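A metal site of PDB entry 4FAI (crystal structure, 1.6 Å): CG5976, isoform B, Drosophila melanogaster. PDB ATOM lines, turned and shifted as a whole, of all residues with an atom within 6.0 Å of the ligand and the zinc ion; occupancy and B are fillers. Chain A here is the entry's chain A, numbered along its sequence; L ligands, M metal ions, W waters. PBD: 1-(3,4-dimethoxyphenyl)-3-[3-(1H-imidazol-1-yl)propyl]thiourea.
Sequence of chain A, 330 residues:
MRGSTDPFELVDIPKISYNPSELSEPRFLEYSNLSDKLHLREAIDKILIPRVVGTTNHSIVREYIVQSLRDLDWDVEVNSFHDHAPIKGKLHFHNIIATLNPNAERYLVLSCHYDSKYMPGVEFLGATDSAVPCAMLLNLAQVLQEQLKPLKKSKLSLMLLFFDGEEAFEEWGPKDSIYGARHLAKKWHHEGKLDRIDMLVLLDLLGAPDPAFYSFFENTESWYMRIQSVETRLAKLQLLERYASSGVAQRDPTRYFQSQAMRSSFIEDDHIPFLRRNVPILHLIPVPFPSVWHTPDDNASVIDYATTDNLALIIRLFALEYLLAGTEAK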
ATOM      1  N   HIS A 113      25.691  17.026 -16.626  1.00  0.00           N
ATOM      2  CA  HIS A 113      25.520  16.762 -18.043  1.00  0.00           C
ATOM      3  C   HIS A 113      26.664  17.318 -18.880  1.00  0.00           C
ATOM      4  O   HIS A 113      27.192  18.361 -18.552  1.00  0.00           O
ATOM      5  CB  HIS A 113      24.137  17.238 -18.571  1.00  0.00           C
ATOM      6  CG  HIS A 113      23.996  18.712 -18.794  1.00  0.00           C
ATOM      7  ND1 HIS A 113      24.213  19.285 -20.022  1.00  0.00           N
ATOM      8  CD2 HIS A 113      23.600  19.711 -17.961  1.00  0.00           C
ATOM      9  CE1 HIS A 113      24.017  20.593 -19.924  1.00  0.00           C
ATOM     10  NE2 HIS A 113      23.599  20.863 -18.705  1.00  0.00           N
ATOM     11  N   LYS A 117      23.441  22.989 -24.974  1.00  0.00           N
ATOM     12  CA  LYS A 117      22.161  23.322 -25.586  1.00  0.00           C
ATOM     13  C   LYS A 117      22.312  23.806 -27.032  1.00  0.00           C
ATOM     14  O   LYS A 117      23.155  24.626 -27.347  1.00  0.00           O
ATOM     15  CB  LYS A 117      21.452  24.382 -24.778  1.00  0.00           C
ATOM     16  CG  LYS A 117      20.038  24.713 -25.262  1.00  0.00           C
ATOM     17  CD  LYS A 117      19.261  25.494 -24.205  1.00  0.00           C
ATOM     18  CE  LYS A 117      17.848  25.886 -24.702  1.00  0.00           C
ATOM     19  NZ  LYS A 117      16.960  24.784 -24.964  1.00  0.00           N
ATOM     20  N   PHE A 124      26.601  28.312 -28.477  1.00  0.00           N
ATOM     21  CA  PHE A 124      26.338  28.372 -27.049  1.00  0.00           C
ATOM     22  C   PHE A 124      27.334  27.463 -26.353  1.00  0.00           C
ATOM     23  O   PHE A 124      27.348  26.265 -26.585  1.00  0.00           O
ATOM     24  CB  PHE A 124      24.914  27.923 -26.741  1.00  0.00           C
ATOM     25  CG  PHE A 124      24.627  27.838 -25.281  1.00  0.00           C
ATOM     26  CD1 PHE A 124      24.549  28.985 -24.513  1.00  0.00           C
ATOM     27  CD2 PHE A 124      24.459  26.596 -24.669  1.00  0.00           C
ATOM     28  CE1 PHE A 124      24.251  28.910 -23.151  1.00  0.00           C
ATOM     29  CE2 PHE A 124      24.180  26.509 -23.302  1.00  0.00           C
ATOM     30  CZ  PHE A 124      24.095  27.658 -22.547  1.00  0.00           C
ATOM     31  N   ASP A 129      26.858  25.540 -17.496  1.00  0.00           N
ATOM     32  CA  ASP A 129      25.756  24.650 -17.854  1.00  0.00           C
ATOM     33  C   ASP A 129      26.137  23.667 -18.977  1.00  0.00           C
ATOM     34  O   ASP A 129      25.663  23.791 -20.148  1.00  0.00           O
ATOM     35  CB  ASP A 129      24.576  25.563 -18.288  1.00  0.00           C
ATOM     36  CG  ASP A 129      23.290  24.838 -18.589  1.00  0.00           C
ATOM     37  OD1 ASP A 129      23.129  23.633 -18.331  1.00  0.00           O
ATOM     38  OD2 ASP A 129      22.363  25.515 -19.107  1.00  0.00           O
ATOM     39  N   SER A 130      26.991  22.677 -18.718  1.00  0.00           N
ATOM     40  CA  SER A 130      27.646  22.356 -17.455  1.00  0.00           C
ATOM     41  C   SER A 130      29.123  21.989 -17.630  1.00  0.00           C
ATOM     42  O   SER A 130      29.655  21.040 -17.029  1.00  0.00           O
ATOM     43  CB  SER A 130      26.875  21.214 -16.755  1.00  0.00           C
ATOM     44  OG  SER A 130      25.692  21.743 -16.192  1.00  0.00           O
ATOM     45  N   GLU A 166      20.820  16.211 -21.733  1.00  0.00           N
ATOM     46  CA  GLU A 166      20.031  16.947 -20.752  1.00  0.00           C
ATOM     47  C   GLU A 166      19.150  18.038 -21.398  1.00  0.00           C
ATOM     48  O   GLU A 166      17.995  18.195 -21.014  1.00  0.00           O
ATOM     49  CB  GLU A 166      20.918  17.550 -19.671  1.00  0.00           C
ATOM     50  CG  GLU A 166      20.161  18.085 -18.479  1.00  0.00           C
ATOM     51  CD  GLU A 166      19.841  19.579 -18.546  1.00  0.00           C
ATOM     52  OE1 GLU A 166      20.137  20.240 -19.578  1.00  0.00           O
ATOM     53  OE2 GLU A 166      19.284  20.085 -17.555  1.00  0.00           O
ATOM     54  N   GLU A 167      19.700  18.777 -22.363  1.00  0.00           N
ATOM     55  CA  GLU A 167      19.033  19.965 -22.876  1.00  0.00           C
ATOM     56  C   GLU A 167      17.980  19.648 -23.918  1.00  0.00           C
ATOM     57  O   GLU A 167      18.124  18.724 -24.700  1.00  0.00           O
ATOM     58  CB  GLU A 167      20.050  20.935 -23.473  1.00  0.00           C
ATOM     59  CG  GLU A 167      21.095  21.387 -22.466  1.00  0.00           C
ATOM     60  CD  GLU A 167      20.638  22.464 -21.552  1.00  0.00           C
ATOM     61  OE1 GLU A 167      21.504  23.025 -20.866  1.00  0.00           O
ATOM     62  OE2 GLU A 167      19.405  22.755 -21.474  1.00  0.00           O
ATOM     63  N   TRP A 172      11.674  22.996 -23.729  1.00  0.00           N
ATOM     64  CA  TRP A 172      11.770  22.082 -22.590  1.00  0.00           C
ATOM     65  C   TRP A 172      10.387  21.542 -22.257  1.00  0.00           C
ATOM     66  O   TRP A 172       9.457  22.319 -22.047  1.00  0.00           O
ATOM     67  CB  TRP A 172      12.358  22.779 -21.356  1.00  0.00           C
ATOM     68  CG  TRP A 172      12.599  21.860 -20.164  1.00  0.00           C
ATOM     69  CD1 TRP A 172      11.679  21.437 -19.241  1.00  0.00           C
ATOM     70  CD2 TRP A 172      13.842  21.264 -19.788  1.00  0.00           C
ATOM     71  NE1 TRP A 172      12.284  20.611 -18.313  1.00  0.00           N
ATOM     72  CE2 TRP A 172      13.609  20.489 -18.625  1.00  0.00           C
ATOM     73  CE3 TRP A 172      15.139  21.306 -20.314  1.00  0.00           C
ATOM     74  CZ2 TRP A 172      14.628  19.780 -17.984  1.00  0.00           C
ATOM     75  CZ3 TRP A 172      16.141  20.614 -19.692  1.00  0.00           C
ATOM     76  CH2 TRP A 172      15.879  19.837 -18.546  1.00  0.00           C
ATOM     77  N   ASP A 204      24.824  21.297 -11.244  1.00  0.00           N
ATOM     78  CA  ASP A 204      24.349  21.992 -12.454  1.00  0.00           C
ATOM     79  C   ASP A 204      24.468  23.501 -12.206  1.00  0.00           C
ATOM     80  O   ASP A 204      24.268  23.952 -11.083  1.00  0.00           O
ATOM     81  CB  ASP A 204      22.908  21.591 -12.786  1.00  0.00           C
ATOM     82  CG  ASP A 204      22.561  21.796 -14.260  1.00  0.00           C
ATOM     83  OD1 ASP A 204      23.336  22.455 -14.986  1.00  0.00           O
ATOM     84  OD2 ASP A 204      21.520  21.272 -14.707  1.00  0.00           O
ATOM     85  N   LEU A 205      24.801  24.247 -13.250  1.00  0.00           N
ATOM     86  CA  LEU A 205      24.863  25.725 -13.222  1.00  0.00           C
ATOM     87  C   LEU A 205      25.862  26.278 -12.185  1.00  0.00           C
ATOM     88  O   LEU A 205      25.549  27.200 -11.436  1.00  0.00           O
ATOM     89  CB  LEU A 205      23.433  26.270 -13.020  1.00  0.00           C
ATOM     90  CG  LEU A 205      22.345  25.716 -13.936  1.00  0.00           C
ATOM     91  CD1 LEU A 205      21.065  26.499 -13.677  1.00  0.00           C
ATOM     92  CD2 LEU A 205      22.698  25.714 -15.449  1.00  0.00           C
ATOM     93  N   PHE A 266       9.973  22.732  -7.775  1.00  0.00           N
ATOM     94  CA  PHE A 266       9.799  21.678  -8.773  1.00  0.00           C
ATOM     95  C   PHE A 266      10.742  21.930  -9.938  1.00  0.00           C
ATOM     96  O   PHE A 266      10.298  21.974 -11.100  1.00  0.00           O
ATOM     97  CB  PHE A 266       8.333  21.620  -9.226  1.00  0.00           C
ATOM     98  CG  PHE A 266       7.382  21.224  -8.126  1.00  0.00           C
ATOM     99  CD1 PHE A 266       6.583  22.181  -7.502  1.00  0.00           C
ATOM    100  CD2 PHE A 266       7.314  19.906  -7.696  1.00  0.00           C
ATOM    101  CE1 PHE A 266       5.706  21.813  -6.476  1.00  0.00           C
ATOM    102  CE2 PHE A 266       6.442  19.530  -6.667  1.00  0.00           C
ATOM    103  CZ  PHE A 266       5.635  20.485  -6.063  1.00  0.00           C
ATOM    104  N   ILE A 267      12.035  22.101  -9.622  1.00  0.00           N
ATOM    105  CA  ILE A 267      13.061  22.312 -10.669  1.00  0.00           C
ATOM    106  C   ILE A 267      13.379  20.998 -11.394  1.00  0.00           C
ATOM    107  O   ILE A 267      13.798  20.012 -10.766  1.00  0.00           O
ATOM    108  CB  ILE A 267      14.394  22.867 -10.143  1.00  0.00           C
ATOM    109  CG1 ILE A 267      14.175  24.196  -9.394  1.00  0.00           C
ATOM    110  CG2 ILE A 267      15.377  23.050 -11.319  1.00  0.00           C
ATOM    111  CD1 ILE A 267      15.427  24.726  -8.700  1.00  0.00           C
ATOM    112  N   GLU A 268      13.185  20.985 -12.700  1.00  0.00           N
ATOM    113  CA  GLU A 268      13.407  19.776 -13.475  1.00  0.00           C
ATOM    114  C   GLU A 268      14.854  19.694 -13.983  1.00  0.00           C
ATOM    115  O   GLU A 268      15.450  20.713 -14.346  1.00  0.00           O
ATOM    116  CB  GLU A 268      12.461  19.744 -14.646  1.00  0.00           C
ATOM    117  CG  GLU A 268      10.998  19.875 -14.177  1.00  0.00           C
ATOM    118  CD  GLU A 268      10.015  19.627 -15.282  1.00  0.00           C
ATOM    119  OE1 GLU A 268      10.399  19.783 -16.471  1.00  0.00           O
ATOM    120  OE2 GLU A 268       8.864  19.272 -14.954  1.00  0.00           O
ATOM    121  N   ASP A 269      15.430  18.500 -13.959  1.00  0.00           N
ATOM    122  CA  ASP A 269      16.818  18.283 -14.365  1.00  0.00           C
ATOM    123  C   ASP A 269      17.002  16.761 -14.532  1.00  0.00           C
ATOM    124  O   ASP A 269      16.025  15.977 -14.407  1.00  0.00           O
ATOM    125  CB  ASP A 269      17.776  18.850 -13.296  1.00  0.00           C
ATOM    126  CG  ASP A 269      19.144  19.270 -13.848  1.00  0.00           C
ATOM    127  OD1 ASP A 269      19.538  18.887 -14.971  1.00  0.00           O
ATOM    128  OD2 ASP A 269      19.868  20.016 -13.123  1.00  0.00           O
ATOM    129  N   ILE A 285      22.342  22.884  -7.357  1.00  0.00           N
ATOM    130  CA  ILE A 285      21.989  23.887  -8.359  1.00  0.00           C
ATOM    131  C   ILE A 285      21.600  25.182  -7.599  1.00  0.00           C
ATOM    132  O   ILE A 285      20.809  25.137  -6.653  1.00  0.00           O
ATOM    133  CB  ILE A 285      20.856  23.382  -9.298  1.00  0.00           C
ATOM    134  CG1 ILE A 285      20.627  24.345 -10.470  1.00  0.00           C
ATOM    135  CG2 ILE A 285      19.453  23.139  -8.553  1.00  0.00           C
ATOM    136  CD1 ILE A 285      19.593  23.825 -11.498  1.00  0.00           C
ATOM    137  N   PRO A 286      22.171  26.329  -7.990  1.00  0.00           N
ATOM    138  CA  PRO A 286      21.885  27.570  -7.272  1.00  0.00           C
ATOM    139  C   PRO A 286      20.480  28.076  -7.627  1.00  0.00           C
ATOM    140  O   PRO A 286      19.968  27.786  -8.707  1.00  0.00           O
ATOM    141  CB  PRO A 286      22.953  28.544  -7.773  1.00  0.00           C
ATOM    142  CG  PRO A 286      23.768  27.796  -8.762  1.00  0.00           C
ATOM    143  CD  PRO A 286      23.041  26.553  -9.162  1.00  0.00           C
ATOM    144  N   VAL A 287      19.864  28.773  -6.673  1.00  0.00           N
ATOM    145  CA  VAL A 287      18.599  29.456  -6.897  1.00  0.00           C
ATOM    146  C   VAL A 287      18.730  30.861  -6.270  1.00  0.00           C
ATOM    147  O   VAL A 287      18.981  31.004  -5.074  1.00  0.00           O
ATOM    148  CB  VAL A 287      17.394  28.693  -6.233  1.00  0.00           C
ATOM    149  CG1 VAL A 287      16.066  29.438  -6.508  1.00  0.00           C
ATOM    150  CG2 VAL A 287      17.318  27.279  -6.744  1.00  0.00           C
ATOM    151  N   PRO A 288      18.618  31.897  -7.093  1.00  0.00           N
ATOM    152  CA  PRO A 288      18.294  31.883  -8.508  1.00  0.00           C
ATOM    153  C   PRO A 288      19.389  31.285  -9.429  1.00  0.00           C
ATOM    154  O   PRO A 288      20.545  31.220  -9.056  1.00  0.00           O
ATOM    155  CB  PRO A 288      18.108  33.380  -8.809  1.00  0.00           C
ATOM    156  CG  PRO A 288      19.101  34.045  -7.910  1.00  0.00           C
ATOM    157  CD  PRO A 288      18.986  33.250  -6.634  1.00  0.00           C
ATOM    158  N   PHE A 289      19.001  30.850 -10.628  1.00  0.00           N
ATOM    159  CA  PHE A 289      19.979  30.437 -11.644  1.00  0.00           C
ATOM    160  C   PHE A 289      20.844  31.648 -11.998  1.00  0.00           C
ATOM    161  O   PHE A 289      20.391  32.784 -11.887  1.00  0.00           O
ATOM    162  CB  PHE A 289      19.307  29.976 -12.949  1.00  0.00           C
ATOM    163  CG  PHE A 289      18.518  28.684 -12.863  1.00  0.00           C
ATOM    164  CD1 PHE A 289      18.412  27.947 -11.694  1.00  0.00           C
ATOM    165  CD2 PHE A 289      17.904  28.197 -14.009  1.00  0.00           C
ATOM    166  CE1 PHE A 289      17.674  26.789 -11.673  1.00  0.00           C
ATOM    167  CE2 PHE A 289      17.181  27.042 -14.003  1.00  0.00           C
ATOM    168  CZ  PHE A 289      17.077  26.311 -12.826  1.00  0.00           C
ATOM    169  N   TRP A 293      21.923  32.471 -17.771  1.00  0.00           N
ATOM    170  CA  TRP A 293      21.367  31.159 -18.072  1.00  0.00           C
ATOM    171  C   TRP A 293      20.756  31.088 -19.470  1.00  0.00           C
ATOM    172  O   TRP A 293      19.862  31.895 -19.801  1.00  0.00           O
ATOM    173  CB  TRP A 293      20.317  30.775 -17.024  1.00  0.00           C
ATOM    174  CG  TRP A 293      19.724  29.412 -17.218  1.00  0.00           C
ATOM    175  CD1 TRP A 293      20.327  28.190 -16.946  1.00  0.00           C
ATOM    176  CD2 TRP A 293      18.430  29.119 -17.696  1.00  0.00           C
ATOM    177  NE1 TRP A 293      19.461  27.174 -17.251  1.00  0.00           N
ATOM    178  CE2 TRP A 293      18.277  27.712 -17.694  1.00  0.00           C
ATOM    179  CE3 TRP A 293      17.334  29.906 -18.103  1.00  0.00           C
ATOM    180  CZ2 TRP A 293      17.115  27.093 -18.112  1.00  0.00           C
ATOM    181  CZ3 TRP A 293      16.187  29.287 -18.488  1.00  0.00           C
ATOM    182  CH2 TRP A 293      16.067  27.896 -18.500  1.00  0.00           C
ATOM    183  N   HIS A 294      21.229  30.132 -20.270  1.00  0.00           N
ATOM    184  CA  HIS A 294      20.725  29.912 -21.640  1.00  0.00           C
ATOM    185  C   HIS A 294      20.849  31.142 -22.556  1.00  0.00           C
ATOM    186  O   HIS A 294      20.041  31.344 -23.453  1.00  0.00           O
ATOM    187  CB  HIS A 294      19.305  29.329 -21.630  1.00  0.00           C
ATOM    188  CG  HIS A 294      19.255  27.891 -21.177  1.00  0.00           C
ATOM    189  ND1 HIS A 294      18.113  27.113 -21.231  1.00  0.00           N
ATOM    190  CD2 HIS A 294      20.237  27.088 -20.696  1.00  0.00           C
ATOM    191  CE1 HIS A 294      18.387  25.901 -20.774  1.00  0.00           C
ATOM    192  NE2 HIS A 294      19.667  25.860 -20.445  1.00  0.00           N
HETATM  193  CAA PBD L   1      15.503  31.204 -15.245  1.00  0.00           C
HETATM  194  CAB PBD L   1      14.304  28.759 -10.335  1.00  0.00           C
HETATM  195  SAC PBD L   1      11.732  23.443 -14.265  1.00  0.00           S
HETATM  196  CAD PBD L   1      20.187  23.416 -16.830  1.00  0.00           C
HETATM  197  CAE PBD L   1      13.455  27.701 -15.154  1.00  0.00           C
HETATM  198  CAF PBD L   1      14.234  28.847 -15.150  1.00  0.00           C
HETATM  199  CAG PBD L   1      19.114  23.011 -16.130  1.00  0.00           C
HETATM  200  CAH PBD L   1      18.457  23.428 -18.169  1.00  0.00           C
HETATM  201  CAI PBD L   1      13.488  27.703 -12.756  1.00  0.00           C
HETATM  202  CAJ PBD L   1      16.023  23.728 -15.761  1.00  0.00           C
HETATM  203  CAK PBD L   1      14.572  23.432 -15.318  1.00  0.00           C
HETATM  204  CAL PBD L   1      16.644  22.640 -16.609  1.00  0.00           C
HETATM  205  NAM PBD L   1      19.781  23.678 -18.106  1.00  0.00           N
HETATM  206  NAN PBD L   1      14.021  24.689 -14.807  1.00  0.00           N
HETATM  207  NAO PBD L   1      12.334  26.008 -13.915  1.00  0.00           N
HETATM  208  OAP PBD L   1      15.389  30.579 -13.919  1.00  0.00           O
HETATM  209  OAQ PBD L   1      14.653  29.447 -11.570  1.00  0.00           O
HETATM  210  CAR PBD L   1      12.770  24.819 -14.344  1.00  0.00           C
HETATM  211  CAS PBD L   1      13.094  27.108 -13.951  1.00  0.00           C
HETATM  212  CAT PBD L   1      14.632  29.435 -13.951  1.00  0.00           C
HETATM  213  CAU PBD L   1      14.246  28.854 -12.741  1.00  0.00           C
HETATM  214  NAV PBD L   1      18.052  23.026 -16.970  1.00  0.00           N
HETATM  215 ZN    ZN M   1      20.844  24.397 -19.607  1.00  0.00          ZN
HETATM  216  O   HOH W   1       9.363  27.555 -13.159  1.00  0.00           O
HETATM  217  O   HOH W   2      16.381  31.531 -11.344  1.00  0.00           O
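The backbone NH of Glu 268 lies close to a sulfur (SAC) of the ligand (3.3 Å).
The side-chain carboxylate of Asp 129 lies within hydrogen-bond range of a ring nitrogen (NE2) of His 113 (2.8 Å). NE2 of His 294 sits close to NE1 of Trp 293 (3.5 Å). OE1 of Glu 268 lies within hydrogen-bond range of NE1 of Trp 172 (2.8 Å). The side-chain carboxylate (OD2) of Asp 204 lies close to the side-chain carboxylate (OD2) of Asp 269 (2.6 Å). The side-chain carboxylate of Asp 204 sits at hydrogen-bond distance from the side-chain hydroxyl of Ser 130, at 2.7 Å.
A nitrogen (NAV) of the ligand sits close to the side-chain carboxylate of Glu 166 (3.2 Å). The backbone carbonyl oxygen (O) of Phe 266 lies close to a sulfur (SAC) of the ligand. Trp 172 touches the ligand. Asp 204 touches the ligand. CD2 of Leu 205 touches CAD of the ligand (3.7 Å). Ile 267 touches the ligand (CA to SAC, 3.997 Å). Phe 289 touches the ligand (CD2 to OAP, 3.5 Å). NE1 of Trp 293 touches NAM of the ligand, 3.6 Å away. Hydrophobic or aromatic side chains within 4 Å of the ligand: Trp 172, Leu 205, Phe 289, Trp 293 and His 294. Of the 21 residues printed, 12 come within 4 Å of the ligand.
Trp 293 touches the zinc ion. Of the 21 residues printed, 4 come within 4 Å of the zinc ion.
The zinc ion is bound by OD2 of Asp 129, NAM of the ligand, OE1 of Glu 167 and NE2 of His 294. Slightly farther from the zinc ion lies OD1 of Asp 129 (2.7 Å).
Water W2 lies within hydrogen-bond range of OAQ of the ligand and N of Phe 289.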
